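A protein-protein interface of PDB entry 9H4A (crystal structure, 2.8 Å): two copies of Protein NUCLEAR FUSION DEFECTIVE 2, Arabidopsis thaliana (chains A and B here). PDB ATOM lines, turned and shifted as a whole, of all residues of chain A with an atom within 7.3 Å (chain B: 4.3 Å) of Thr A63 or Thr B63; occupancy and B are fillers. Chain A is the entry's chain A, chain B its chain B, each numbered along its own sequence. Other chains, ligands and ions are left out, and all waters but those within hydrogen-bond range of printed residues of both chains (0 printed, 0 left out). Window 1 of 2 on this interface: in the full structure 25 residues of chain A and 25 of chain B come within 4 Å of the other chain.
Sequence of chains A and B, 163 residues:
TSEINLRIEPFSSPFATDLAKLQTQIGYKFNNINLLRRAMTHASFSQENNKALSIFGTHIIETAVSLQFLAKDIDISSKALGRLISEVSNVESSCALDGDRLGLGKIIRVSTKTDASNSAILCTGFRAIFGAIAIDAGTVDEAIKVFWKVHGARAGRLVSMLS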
ATOM      1  N   ILE A  55      -3.646 -32.324  -6.351  1.00  0.00           N
ATOM      2  CA  ILE A  55      -2.453 -31.573  -6.727  1.00  0.00           C
ATOM      3  C   ILE A  55      -2.246 -30.394  -5.785  1.00  0.00           C
ATOM      4  O   ILE A  55      -1.111 -30.062  -5.421  1.00  0.00           O
ATOM      5  CB  ILE A  55      -2.552 -31.121  -8.195  1.00  0.00           C
ATOM      6  CG1 ILE A  55      -2.743 -32.332  -9.110  1.00  0.00           C
ATOM      7  CG2 ILE A  55      -1.314 -30.337  -8.598  1.00  0.00           C
ATOM      8  CD1 ILE A  55      -2.835 -31.982 -10.579  1.00  0.00           C
ATOM      9  N   PHE A  56      -3.337 -29.743  -5.376  1.00  0.00           N
ATOM     10  CA  PHE A  56      -3.243 -28.666  -4.395  1.00  0.00           C
ATOM     11  C   PHE A  56      -2.693 -29.186  -3.073  1.00  0.00           C
ATOM     12  O   PHE A  56      -1.763 -28.605  -2.501  1.00  0.00           O
ATOM     13  CB  PHE A  56      -4.621 -28.029  -4.198  1.00  0.00           C
ATOM     14  CG  PHE A  56      -4.595 -26.712  -3.467  1.00  0.00           C
ATOM     15  CD1 PHE A  56      -3.398 -26.081  -3.168  1.00  0.00           C
ATOM     16  CD2 PHE A  56      -5.777 -26.107  -3.076  1.00  0.00           C
ATOM     17  CE1 PHE A  56      -3.382 -24.875  -2.497  1.00  0.00           C
ATOM     18  CE2 PHE A  56      -5.768 -24.901  -2.404  1.00  0.00           C
ATOM     19  CZ  PHE A  56      -4.568 -24.284  -2.114  1.00  0.00           C
ATOM     20  N   GLY A  57      -3.254 -30.290  -2.576  1.00  0.00           N
ATOM     21  CA  GLY A  57      -2.815 -30.826  -1.300  1.00  0.00           C
ATOM     22  C   GLY A  57      -1.370 -31.282  -1.302  1.00  0.00           C
ATOM     23  O   GLY A  57      -0.711 -31.266  -0.261  1.00  0.00           O
ATOM     24  N   THR A  58      -0.858 -31.692  -2.464  1.00  0.00           N
ATOM     25  CA  THR A  58       0.540 -32.107  -2.548  1.00  0.00           C
ATOM     26  C   THR A  58       1.474 -30.937  -2.263  1.00  0.00           C
ATOM     27  O   THR A  58       2.430 -31.064  -1.490  1.00  0.00           O
ATOM     28  CB  THR A  58       0.832 -32.706  -3.924  1.00  0.00           C
ATOM     29  OG1 THR A  58       0.044 -33.887  -4.112  1.00  0.00           O
ATOM     30  CG2 THR A  58       2.304 -33.066  -4.045  1.00  0.00           C
ATOM     31  N   HIS A  59       1.204 -29.782  -2.875  1.00  0.00           N
ATOM     32  CA  HIS A  59       2.073 -28.626  -2.678  1.00  0.00           C
ATOM     33  C   HIS A  59       1.887 -28.005  -1.301  1.00  0.00           C
ATOM     34  O   HIS A  59       2.820 -27.391  -0.771  1.00  0.00           O
ATOM     35  CB  HIS A  59       1.821 -27.594  -3.776  1.00  0.00           C
ATOM     36  CG  HIS A  59       2.030 -28.127  -5.158  1.00  0.00           C
ATOM     37  ND1 HIS A  59       3.177 -28.791  -5.533  1.00  0.00           N
ATOM     38  CD2 HIS A  59       1.235 -28.100  -6.255  1.00  0.00           C
ATOM     39  CE1 HIS A  59       3.082 -29.148  -6.801  1.00  0.00           C
ATOM     40  NE2 HIS A  59       1.914 -28.740  -7.262  1.00  0.00           N
ATOM     41  N   ILE A  60       0.701 -28.150  -0.707  1.00  0.00           N
ATOM     42  CA  ILE A  60       0.500 -27.683   0.662  1.00  0.00           C
ATOM     43  C   ILE A  60       1.372 -28.481   1.622  1.00  0.00           C
ATOM     44  O   ILE A  60       2.006 -27.920   2.525  1.00  0.00           O
ATOM     45  CB  ILE A  60      -0.989 -27.762   1.045  1.00  0.00           C
ATOM     46  CG1 ILE A  60      -1.812 -26.795   0.192  1.00  0.00           C
ATOM     47  CG2 ILE A  60      -1.180 -27.462   2.524  1.00  0.00           C
ATOM     48  CD1 ILE A  60      -3.286 -26.782   0.534  1.00  0.00           C
ATOM     49  N   ILE A  61       1.427 -29.801   1.437  1.00  0.00           N
ATOM     50  CA  ILE A  61       2.255 -30.639   2.296  1.00  0.00           C
ATOM     51  C   ILE A  61       3.734 -30.355   2.055  1.00  0.00           C
ATOM     52  O   ILE A  61       4.534 -30.327   2.998  1.00  0.00           O
ATOM     53  CB  ILE A  61       1.910 -32.123   2.074  1.00  0.00           C
ATOM     54  CG1 ILE A  61       0.461 -32.392   2.491  1.00  0.00           C
ATOM     55  CG2 ILE A  61       2.870 -33.020   2.838  1.00  0.00           C
ATOM     56  CD1 ILE A  61      -0.024 -33.789   2.174  1.00  0.00           C
ATOM     57  N   GLU A  62       4.118 -30.126   0.797  1.00  0.00           N
ATOM     58  CA  GLU A  62       5.508 -29.788   0.498  1.00  0.00           C
ATOM     59  C   GLU A  62       5.919 -28.491   1.185  1.00  0.00           C
ATOM     60  O   GLU A  62       7.066 -28.348   1.625  1.00  0.00           O
ATOM     61  CB  GLU A  62       5.712 -29.684  -1.012  1.00  0.00           C
ATOM     62  CG  GLU A  62       5.697 -31.019  -1.734  1.00  0.00           C
ATOM     63  CD  GLU A  62       5.826 -30.868  -3.236  1.00  0.00           C
ATOM     64  OE1 GLU A  62       5.378 -29.832  -3.772  1.00  0.00           O
ATOM     65  OE2 GLU A  62       6.382 -31.782  -3.881  1.00  0.00           O
ATOM     66  N   THR A  63       4.993 -27.536   1.286  1.00  0.00           N
ATOM     67  CA  THR A  63       5.266 -26.293   1.998  1.00  0.00           C
ATOM     68  C   THR A  63       5.244 -26.502   3.509  1.00  0.00           C
ATOM     69  O   THR A  63       6.052 -25.911   4.235  1.00  0.00           O
ATOM     70  CB  THR A  63       4.251 -25.225   1.585  1.00  0.00           C
ATOM     71  OG1 THR A  63       4.447 -24.887   0.207  1.00  0.00           O
ATOM     72  CG2 THR A  63       4.399 -23.973   2.434  1.00  0.00           C
ATOM     73  N   ALA A  64       4.331 -27.347   3.997  1.00  0.00           N
ATOM     74  CA  ALA A  64       4.259 -27.616   5.430  1.00  0.00           C
ATOM     75  C   ALA A  64       5.535 -28.278   5.932  1.00  0.00           C
ATOM     76  O   ALA A  64       6.036 -27.941   7.011  1.00  0.00           O
ATOM     77  CB  ALA A  64       3.044 -28.493   5.735  1.00  0.00           C
ATOM     78  N   VAL A  65       6.075 -29.223   5.161  1.00  0.00           N
ATOM     79  CA  VAL A  65       7.309 -29.896   5.553  1.00  0.00           C
ATOM     80  C   VAL A  65       8.496 -28.949   5.434  1.00  0.00           C
ATOM     81  O   VAL A  65       9.403 -28.957   6.277  1.00  0.00           O
ATOM     82  CB  VAL A  65       7.505 -31.167   4.705  1.00  0.00           C
ATOM     83  CG1 VAL A  65       8.858 -31.799   4.983  1.00  0.00           C
ATOM     84  CG2 VAL A  65       6.388 -32.159   4.977  1.00  0.00           C
ATOM     85  N   SER A  66       8.508 -28.111   4.395  1.00  0.00           N
ATOM     86  CA  SER A  66       9.632 -27.203   4.188  1.00  0.00           C
ATOM     87  C   SER A  66       9.716 -26.162   5.296  1.00  0.00           C
ATOM     88  O   SER A  66      10.814 -25.823   5.755  1.00  0.00           O
ATOM     89  CB  SER A  66       9.513 -26.525   2.825  1.00  0.00           C
ATOM     90  OG  SER A  66       9.481 -27.479   1.779  1.00  0.00           O
ATOM     91  N   LEU A  67       8.569 -25.645   5.742  1.00  0.00           N
ATOM     92  CA  LEU A  67       8.578 -24.609   6.770  1.00  0.00           C
ATOM     93  C   LEU A  67       9.065 -25.156   8.107  1.00  0.00           C
ATOM     94  O   LEU A  67       9.790 -24.469   8.835  1.00  0.00           O
ATOM     95  CB  LEU A  67       7.182 -24.002   6.917  1.00  0.00           C
ATOM     96  CG  LEU A  67       7.036 -22.899   7.967  1.00  0.00           C
ATOM     97  CD1 LEU A  67       7.811 -21.652   7.560  1.00  0.00           C
ATOM     98  CD2 LEU A  67       5.572 -22.569   8.210  1.00  0.00           C
ATOM     99  N   GLN A  68       8.685 -26.390   8.443  1.00  0.00           N
ATOM    100  CA  GLN A  68       9.033 -26.934   9.751  1.00  0.00           C
ATOM    101  C   GLN A  68      10.520 -27.252   9.859  1.00  0.00           C
ATOM    102  O   GLN A  68      11.105 -27.106  10.938  1.00  0.00           O
ATOM    103  CB  GLN A  68       8.196 -28.181  10.041  1.00  0.00           C
ATOM    104  CG  GLN A  68       8.224 -28.627  11.494  1.00  0.00           C
ATOM    105  CD  GLN A  68       7.132 -29.628  11.820  1.00  0.00           C
ATOM    106  OE1 GLN A  68       6.619 -29.663  12.939  1.00  0.00           O
ATOM    107  NE2 GLN A  68       6.771 -30.450  10.842  1.00  0.00           N
ATOM    108  N   PHE A  69      11.150 -27.680   8.764  1.00  0.00           N
ATOM    109  CA  PHE A  69      12.575 -27.990   8.817  1.00  0.00           C
ATOM    110  C   PHE A  69      13.431 -26.739   8.674  1.00  0.00           C
ATOM    111  O   PHE A  69      14.443 -26.595   9.370  1.00  0.00           O
ATOM    112  CB  PHE A  69      12.938 -29.010   7.738  1.00  0.00           C
ATOM    113  CG  PHE A  69      12.507 -30.411   8.063  1.00  0.00           C
ATOM    114  CD1 PHE A  69      13.019 -31.064   9.171  1.00  0.00           C
ATOM    115  CD2 PHE A  69      11.601 -31.076   7.258  1.00  0.00           C
ATOM    116  CE1 PHE A  69      12.627 -32.353   9.476  1.00  0.00           C
ATOM    117  CE2 PHE A  69      11.208 -32.367   7.555  1.00  0.00           C
ATOM    118  CZ  PHE A  69      11.722 -33.005   8.666  1.00  0.00           C
ATOM    119  N   ILE A  85      11.348 -34.001   2.096  1.00  0.00           N
ATOM    120  CA  ILE A  85      10.065 -33.778   1.437  1.00  0.00           C
ATOM    121  C   ILE A  85       9.575 -35.063   0.781  1.00  0.00           C
ATOM    122  O   ILE A  85       8.381 -35.382   0.821  1.00  0.00           O
ATOM    123  CB  ILE A  85      10.176 -32.627   0.419  1.00  0.00           C
ATOM    124  CG1 ILE A  85      10.368 -31.291   1.140  1.00  0.00           C
ATOM    125  CG2 ILE A  85       8.945 -32.571  -0.470  1.00  0.00           C
ATOM    126  CD1 ILE A  85      10.538 -30.114   0.204  1.00  0.00           C
ATOM    127  N   ALA A 134      -8.104 -25.544   2.529  1.00  0.00           N
ATOM    128  CA  ALA A 134      -7.660 -24.193   2.206  1.00  0.00           C
ATOM    129  C   ALA A 134      -8.711 -23.442   1.400  1.00  0.00           C
ATOM    130  O   ALA A 134      -8.940 -22.248   1.629  1.00  0.00           O
ATOM    131  CB  ALA A 134      -6.333 -24.244   1.448  1.00  0.00           C
ATOM    132  N   VAL A 140      -4.190 -20.815   3.417  1.00  0.00           N
ATOM    133  CA  VAL A 140      -3.370 -22.019   3.338  1.00  0.00           C
ATOM    134  C   VAL A 140      -2.749 -22.340   4.693  1.00  0.00           C
ATOM    135  O   VAL A 140      -2.479 -23.509   4.995  1.00  0.00           O
ATOM    136  CB  VAL A 140      -2.304 -21.856   2.237  1.00  0.00           C
ATOM    137  CG1 VAL A 140      -1.398 -23.076   2.164  1.00  0.00           C
ATOM    138  CG2 VAL A 140      -2.972 -21.619   0.894  1.00  0.00           C
ATOM    139  N   ASP A 141      -2.534 -21.324   5.535  1.00  0.00           N
ATOM    140  CA  ASP A 141      -1.960 -21.560   6.857  1.00  0.00           C
ATOM    141  C   ASP A 141      -2.814 -22.521   7.671  1.00  0.00           C
ATOM    142  O   ASP A 141      -2.287 -23.328   8.445  1.00  0.00           O
ATOM    143  CB  ASP A 141      -1.796 -20.236   7.605  1.00  0.00           C
ATOM    144  CG  ASP A 141      -0.729 -19.352   6.999  1.00  0.00           C
ATOM    145  OD1 ASP A 141       0.271 -19.893   6.482  1.00  0.00           O
ATOM    146  OD2 ASP A 141      -0.889 -18.114   7.041  1.00  0.00           O
ATOM    147  N   ILE A 144      -2.044 -26.047   6.669  1.00  0.00           N
ATOM    148  CA  ILE A 144      -0.737 -26.461   7.166  1.00  0.00           C
ATOM    149  C   ILE A 144      -0.821 -26.825   8.643  1.00  0.00           C
ATOM    150  O   ILE A 144      -0.162 -27.765   9.104  1.00  0.00           O
ATOM    151  CB  ILE A 144       0.303 -25.356   6.905  1.00  0.00           C
ATOM    152  CG1 ILE A 144       0.495 -25.156   5.398  1.00  0.00           C
ATOM    153  CG2 ILE A 144       1.626 -25.684   7.576  1.00  0.00           C
ATOM    154  CD1 ILE A 144       1.483 -24.070   5.049  1.00  0.00           C
ATOM    155  N   TRP A 148      -0.134 -30.774  10.202  1.00  0.00           N
ATOM    156  CA  TRP A 148       0.840 -31.032  11.257  1.00  0.00           C
ATOM    157  C   TRP A 148       0.233 -31.833  12.399  1.00  0.00           C
ATOM    158  O   TRP A 148       0.953 -32.544  13.110  1.00  0.00           O
ATOM    159  CB  TRP A 148       1.409 -29.711  11.775  1.00  0.00           C
ATOM    160  CG  TRP A 148       2.449 -29.110  10.878  1.00  0.00           C
ATOM    161  CD1 TRP A 148       3.154 -29.747   9.899  1.00  0.00           C
ATOM    162  CD2 TRP A 148       2.900 -27.749  10.878  1.00  0.00           C
ATOM    163  NE1 TRP A 148       4.018 -28.868   9.291  1.00  0.00           N
ATOM    164  CE2 TRP A 148       3.881 -27.635   9.873  1.00  0.00           C
ATOM    165  CE3 TRP A 148       2.570 -26.617  11.630  1.00  0.00           C
ATOM    166  CZ2 TRP A 148       4.534 -26.435   9.600  1.00  0.00           C
ATOM    167  CZ3 TRP A 148       3.220 -25.427  11.358  1.00  0.00           C
ATOM    168  CH2 TRP A 148       4.190 -25.345  10.351  1.00  0.00           C
ATOM    169  N   PHE B  56      11.993 -23.953  -1.062  1.00  0.00           N
ATOM    170  CA  PHE B  56      10.806 -23.556  -0.313  1.00  0.00           C
ATOM    171  C   PHE B  56       9.947 -22.598  -1.130  1.00  0.00           C
ATOM    172  O   PHE B  56       8.723 -22.758  -1.212  1.00  0.00           O
ATOM    173  CB  PHE B  56      11.224 -22.916   1.013  1.00  0.00           C
ATOM    174  CG  PHE B  56      10.089 -22.701   1.984  1.00  0.00           C
ATOM    175  CD1 PHE B  56       8.858 -23.307   1.795  1.00  0.00           C
ATOM    176  CD2 PHE B  56      10.262 -21.884   3.090  1.00  0.00           C
ATOM    177  CE1 PHE B  56       7.823 -23.102   2.689  1.00  0.00           C
ATOM    178  CE2 PHE B  56       9.230 -21.676   3.986  1.00  0.00           C
ATOM    179  CZ  PHE B  56       8.009 -22.287   3.785  1.00  0.00           C
ATOM    180  N   HIS B  59       7.615 -24.264  -3.837  1.00  0.00           N
ATOM    181  CA  HIS B  59       6.358 -24.855  -3.391  1.00  0.00           C
ATOM    182  C   HIS B  59       5.380 -23.796  -2.897  1.00  0.00           C
ATOM    183  O   HIS B  59       4.163 -24.014  -2.940  1.00  0.00           O
ATOM    184  CB  HIS B  59       6.629 -25.896  -2.306  1.00  0.00           C
ATOM    185  CG  HIS B  59       7.532 -27.005  -2.749  1.00  0.00           C
ATOM    186  ND1 HIS B  59       7.537 -27.487  -4.041  1.00  0.00           N
ATOM    187  CD2 HIS B  59       8.469 -27.717  -2.079  1.00  0.00           C
ATOM    188  CE1 HIS B  59       8.432 -28.452  -4.146  1.00  0.00           C
ATOM    189  NE2 HIS B  59       9.012 -28.611  -2.970  1.00  0.00           N
ATOM    190  N   ILE B  60       5.882 -22.649  -2.433  1.00  0.00           N
ATOM    191  CA  ILE B  60       4.997 -21.553  -2.053  1.00  0.00           C
ATOM    192  C   ILE B  60       4.320 -20.962  -3.284  1.00  0.00           C
ATOM    193  O   ILE B  60       3.133 -20.618  -3.254  1.00  0.00           O
ATOM    194  CB  ILE B  60       5.779 -20.483  -1.267  1.00  0.00           C
ATOM    195  CG1 ILE B  60       6.310 -21.067   0.041  1.00  0.00           C
ATOM    196  CG2 ILE B  60       4.907 -19.269  -0.989  1.00  0.00           C
ATOM    197  CD1 ILE B  60       7.079 -20.073   0.886  1.00  0.00           C
ATOM    198  N   ILE B  61       5.060 -20.840  -4.388  1.00  0.00           N
ATOM    199  CA  ILE B  61       4.474 -20.320  -5.619  1.00  0.00           C
ATOM    200  C   ILE B  61       3.508 -21.335  -6.221  1.00  0.00           C
ATOM    201  O   ILE B  61       2.437 -20.971  -6.721  1.00  0.00           O
ATOM    202  CB  ILE B  61       5.587 -19.926  -6.608  1.00  0.00           C
ATOM    203  CG1 ILE B  61       6.405 -18.764  -6.038  1.00  0.00           C
ATOM    204  CG2 ILE B  61       5.002 -19.559  -7.963  1.00  0.00           C
ATOM    205  CD1 ILE B  61       7.590 -18.364  -6.888  1.00  0.00           C
ATOM    206  N   GLU B  62       3.862 -22.623  -6.174  1.00  0.00           N
ATOM    207  CA  GLU B  62       2.953 -23.661  -6.653  1.00  0.00           C
ATOM    208  C   GLU B  62       1.651 -23.659  -5.864  1.00  0.00           C
ATOM    209  O   GLU B  62       0.571 -23.869  -6.428  1.00  0.00           O
ATOM    210  CB  GLU B  62       3.626 -25.032  -6.566  1.00  0.00           C
ATOM    211  CG  GLU B  62       4.813 -25.215  -7.496  1.00  0.00           C
ATOM    212  CD  GLU B  62       5.593 -26.483  -7.198  1.00  0.00           C
ATOM    213  OE1 GLU B  62       5.468 -27.008  -6.071  1.00  0.00           O
ATOM    214  OE2 GLU B  62       6.329 -26.955  -8.091  1.00  0.00           O
ATOM    215  N   THR B  63       1.734 -23.423  -4.553  1.00  0.00           N
ATOM    216  CA  THR B  63       0.533 -23.395  -3.725  1.00  0.00           C
ATOM    217  C   THR B  63      -0.299 -22.147  -4.001  1.00  0.00           C
ATOM    218  O   THR B  63      -1.534 -22.212  -4.035  1.00  0.00           O
ATOM    219  CB  THR B  63       0.919 -23.470  -2.248  1.00  0.00           C
ATOM    220  OG1 THR B  63       1.685 -24.658  -2.016  1.00  0.00           O
ATOM    221  CG2 THR B  63      -0.318 -23.492  -1.367  1.00  0.00           C
ATOM    222  N   ALA B  64       0.361 -21.005  -4.207  1.00  0.00           N
ATOM    223  CA  ALA B  64      -0.362 -19.767  -4.481  1.00  0.00           C
ATOM    224  C   ALA B  64      -1.122 -19.848  -5.799  1.00  0.00           C
ATOM    225  O   ALA B  64      -2.254 -19.360  -5.901  1.00  0.00           O
ATOM    226  CB  ALA B  64       0.605 -18.585  -4.491  1.00  0.00           C
ATOM    227  N   VAL B  65      -0.516 -20.456  -6.820  1.00  0.00           N
ATOM    228  CA  VAL B  65      -1.201 -20.617  -8.098  1.00  0.00           C
ATOM    229  C   VAL B  65      -2.391 -21.556  -7.949  1.00  0.00           C
ATOM    230  O   VAL B  65      -3.488 -21.277  -8.449  1.00  0.00           O
ATOM    231  CB  VAL B  65      -0.217 -21.111  -9.173  1.00  0.00           C
ATOM    232  CG1 VAL B  65      -0.963 -21.521 -10.433  1.00  0.00           C
ATOM    233  CG2 VAL B  65       0.806 -20.030  -9.487  1.00  0.00           C
ATOM    234  N   SER B  66      -2.199 -22.677  -7.247  1.00  0.00           N
ATOM    235  CA  SER B  66      -3.290 -23.623  -7.042  1.00  0.00           C
ATOM    236  C   SER B  66      -4.418 -23.014  -6.219  1.00  0.00           C
ATOM    237  O   SER B  66      -5.584 -23.379  -6.405  1.00  0.00           O
ATOM    238  CB  SER B  66      -2.769 -24.888  -6.360  1.00  0.00           C
ATOM    239  OG  SER B  66      -1.656 -25.428  -7.048  1.00  0.00           O
ATOM    240  N   LEU B  67      -4.095 -22.090  -5.313  1.00  0.00           N
ATOM    241  CA  LEU B  67      -5.122 -21.507  -4.456  1.00  0.00           C
ATOM    242  C   LEU B  67      -6.043 -20.583  -5.242  1.00  0.00           C
ATOM    243  O   LEU B  67      -7.253 -20.546  -4.991  1.00  0.00           O
ATOM    244  CB  LEU B  67      -4.469 -20.754  -3.296  1.00  0.00           C
ATOM    245  CG  LEU B  67      -5.399 -19.959  -2.378  1.00  0.00           C
ATOM    246  CD1 LEU B  67      -6.413 -20.870  -1.701  1.00  0.00           C
ATOM    247  CD2 LEU B  67      -4.599 -19.182  -1.345  1.00  0.00           C
ATOM    248  N   VAL B 140       2.587 -18.657   5.874  1.00  0.00           N
ATOM    249  CA  VAL B 140       2.770 -18.840   4.437  1.00  0.00           C
ATOM    250  C   VAL B 140       1.848 -17.928   3.634  1.00  0.00           C
ATOM    251  O   VAL B 140       2.233 -17.434   2.570  1.00  0.00           O
ATOM    252  CB  VAL B 140       2.563 -20.325   4.077  1.00  0.00           C
ATOM    253  CG1 VAL B 140       2.581 -20.531   2.568  1.00  0.00           C
ATOM    254  CG2 VAL B 140       3.632 -21.172   4.742  1.00  0.00           C
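Of the 21 printed residues of chain A, 11 touch a printed residue of chain B. Printed residues of chain A that touch a printed residue of chain B: Phe A56, His A59, Ile A60, Glu A62, Thr A63, Ser A66, Leu A67, Ile A85, Val A140, Asp A141 and Ile A144. Along chain A the printed residues that touch a printed residue of chain B span positions 56 to 144. Hydrophobic or aromatic side chains of chain B within 4 Å of the printed part of chain A: Phe B56, His B59, Leu B67 and Val B140. Along chain B the printed residues that touch a printed residue of chain A span positions 56 to 140. Among the printed residues, 21 pairs touch across the chains. Among the printed residues, no Asp or Glu carboxylate lies within 4 Å of a Lys or Arg side-chain nitrogen of the other chain.
Of the printed residues of chain B, His A59 touches Glu B62 and Thr B63. Of the printed residues of chain B, Ile A60 touches Thr B63. Thr A63 touches just these residues of chain B: Phe B56 (3.5 Å), His B59 (3.3 Å), Ile B60 (3.7 Å), Thr B63 (3.6 Å) and Val B140 (3.7 Å). Of the printed residues of chain B, Leu A67 touches Phe B56. Of the printed residues of chain B, Val A140 touches Thr B63 and Leu B67. Trp A148 touches none of the printed residues of chain B. Thr B63 touches just these residues of chain A: Phe A56 (3.5 Å), His A59 (3.2 Å), Ile A60 (3.9 Å), Thr A63 (3.6 Å) and Val A140 (3.7 Å). Of the printed residues of chain A, Val B140 touches Thr A63 (3.7 Å), Asp A141 (2.7 Å) and Ile A144 (3.6 Å).
Phe A56 touches Thr B63, and with the chains exchanged Thr A63 touches Phe B56. Phe A56 touches Leu B67, and with the chains exchanged Leu A67 touches Phe B56. Thr B63 touches its own counterpart, Thr A63. Thr A63 touches Val B140, and with the chains exchanged Val A140 touches Thr B63. Positions printed for both chains: 56, 59, 60, 61, 62, 63, 64, 65, 66, 67 and 140. Of the 21 pairs that touch across the chains among the printed residues, 16 have their exchanged pair printed and touching as well.
ND1 of His A59 sits at hydrogen-bond distance from OE1 of Glu B62 (3.0 Å). The side-chain hydroxyl (OG1) of Thr B63 sits at hydrogen-bond distance from the backbone carbonyl oxygen (O) of His A59 (3.2 Å). ND1 of His B59 is in hydrogen-bond range of OE1 of Glu A62. The side-chain hydroxyl (OG1) of Thr A63 sits at hydrogen-bond distance from the backbone carbonyl oxygen (O) of His B59, 3.3 Å away. The backbone NH of Val B140 sits at hydrogen-bond distance from the side-chain carboxylate of Asp A141, 2.7 Å away.
A ring nitrogen (ND1) of His A59 lies within hydrogen-bond range of the side-chain carboxylate (OE1) of Glu A62. The backbone carbonyl oxygen (O) of His A59 is in hydrogen-bond range of the side-chain hydroxyl (OG1) of Thr A63. The backbone carbonyl oxygen (O) of Glu A62 lies within hydrogen-bond range of the side-chain hydroxyl (OG) of Ser A66, 2.6 Å away. A ring nitrogen (ND1) of His B59 sits at hydrogen-bond distance from the side-chain carboxylate (OE1) of Glu B62, at 2.9 Å. O of His B59 is in hydrogen-bond range of OG1 of Thr B63, 2.7 Å away. O of Glu B62 sits at hydrogen-bond distance from OG of Ser B66 (2.8 Å).
CD1 of Phe A56 touches CB of Ser B66 (3.5 Å). Phe A56 touches Leu B67 (CZ to CA, 3.7 Å). Thr B63 touches Ile A60. OE1 of Glu B62 touches OE1 of Glu A62 (3.6 Å). Phe B56 touches Thr A63 (CE1 to CG2, 3.5 Å). Thr A63 touches Ile B60 (OG1 to N, 3.7 Å). Thr A63 touches Val B140. Leu A67 touches Phe B56. Ile A85 touches His B59 (CD1 to NE2, 3.8 Å). Val A140 touches Thr B63.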
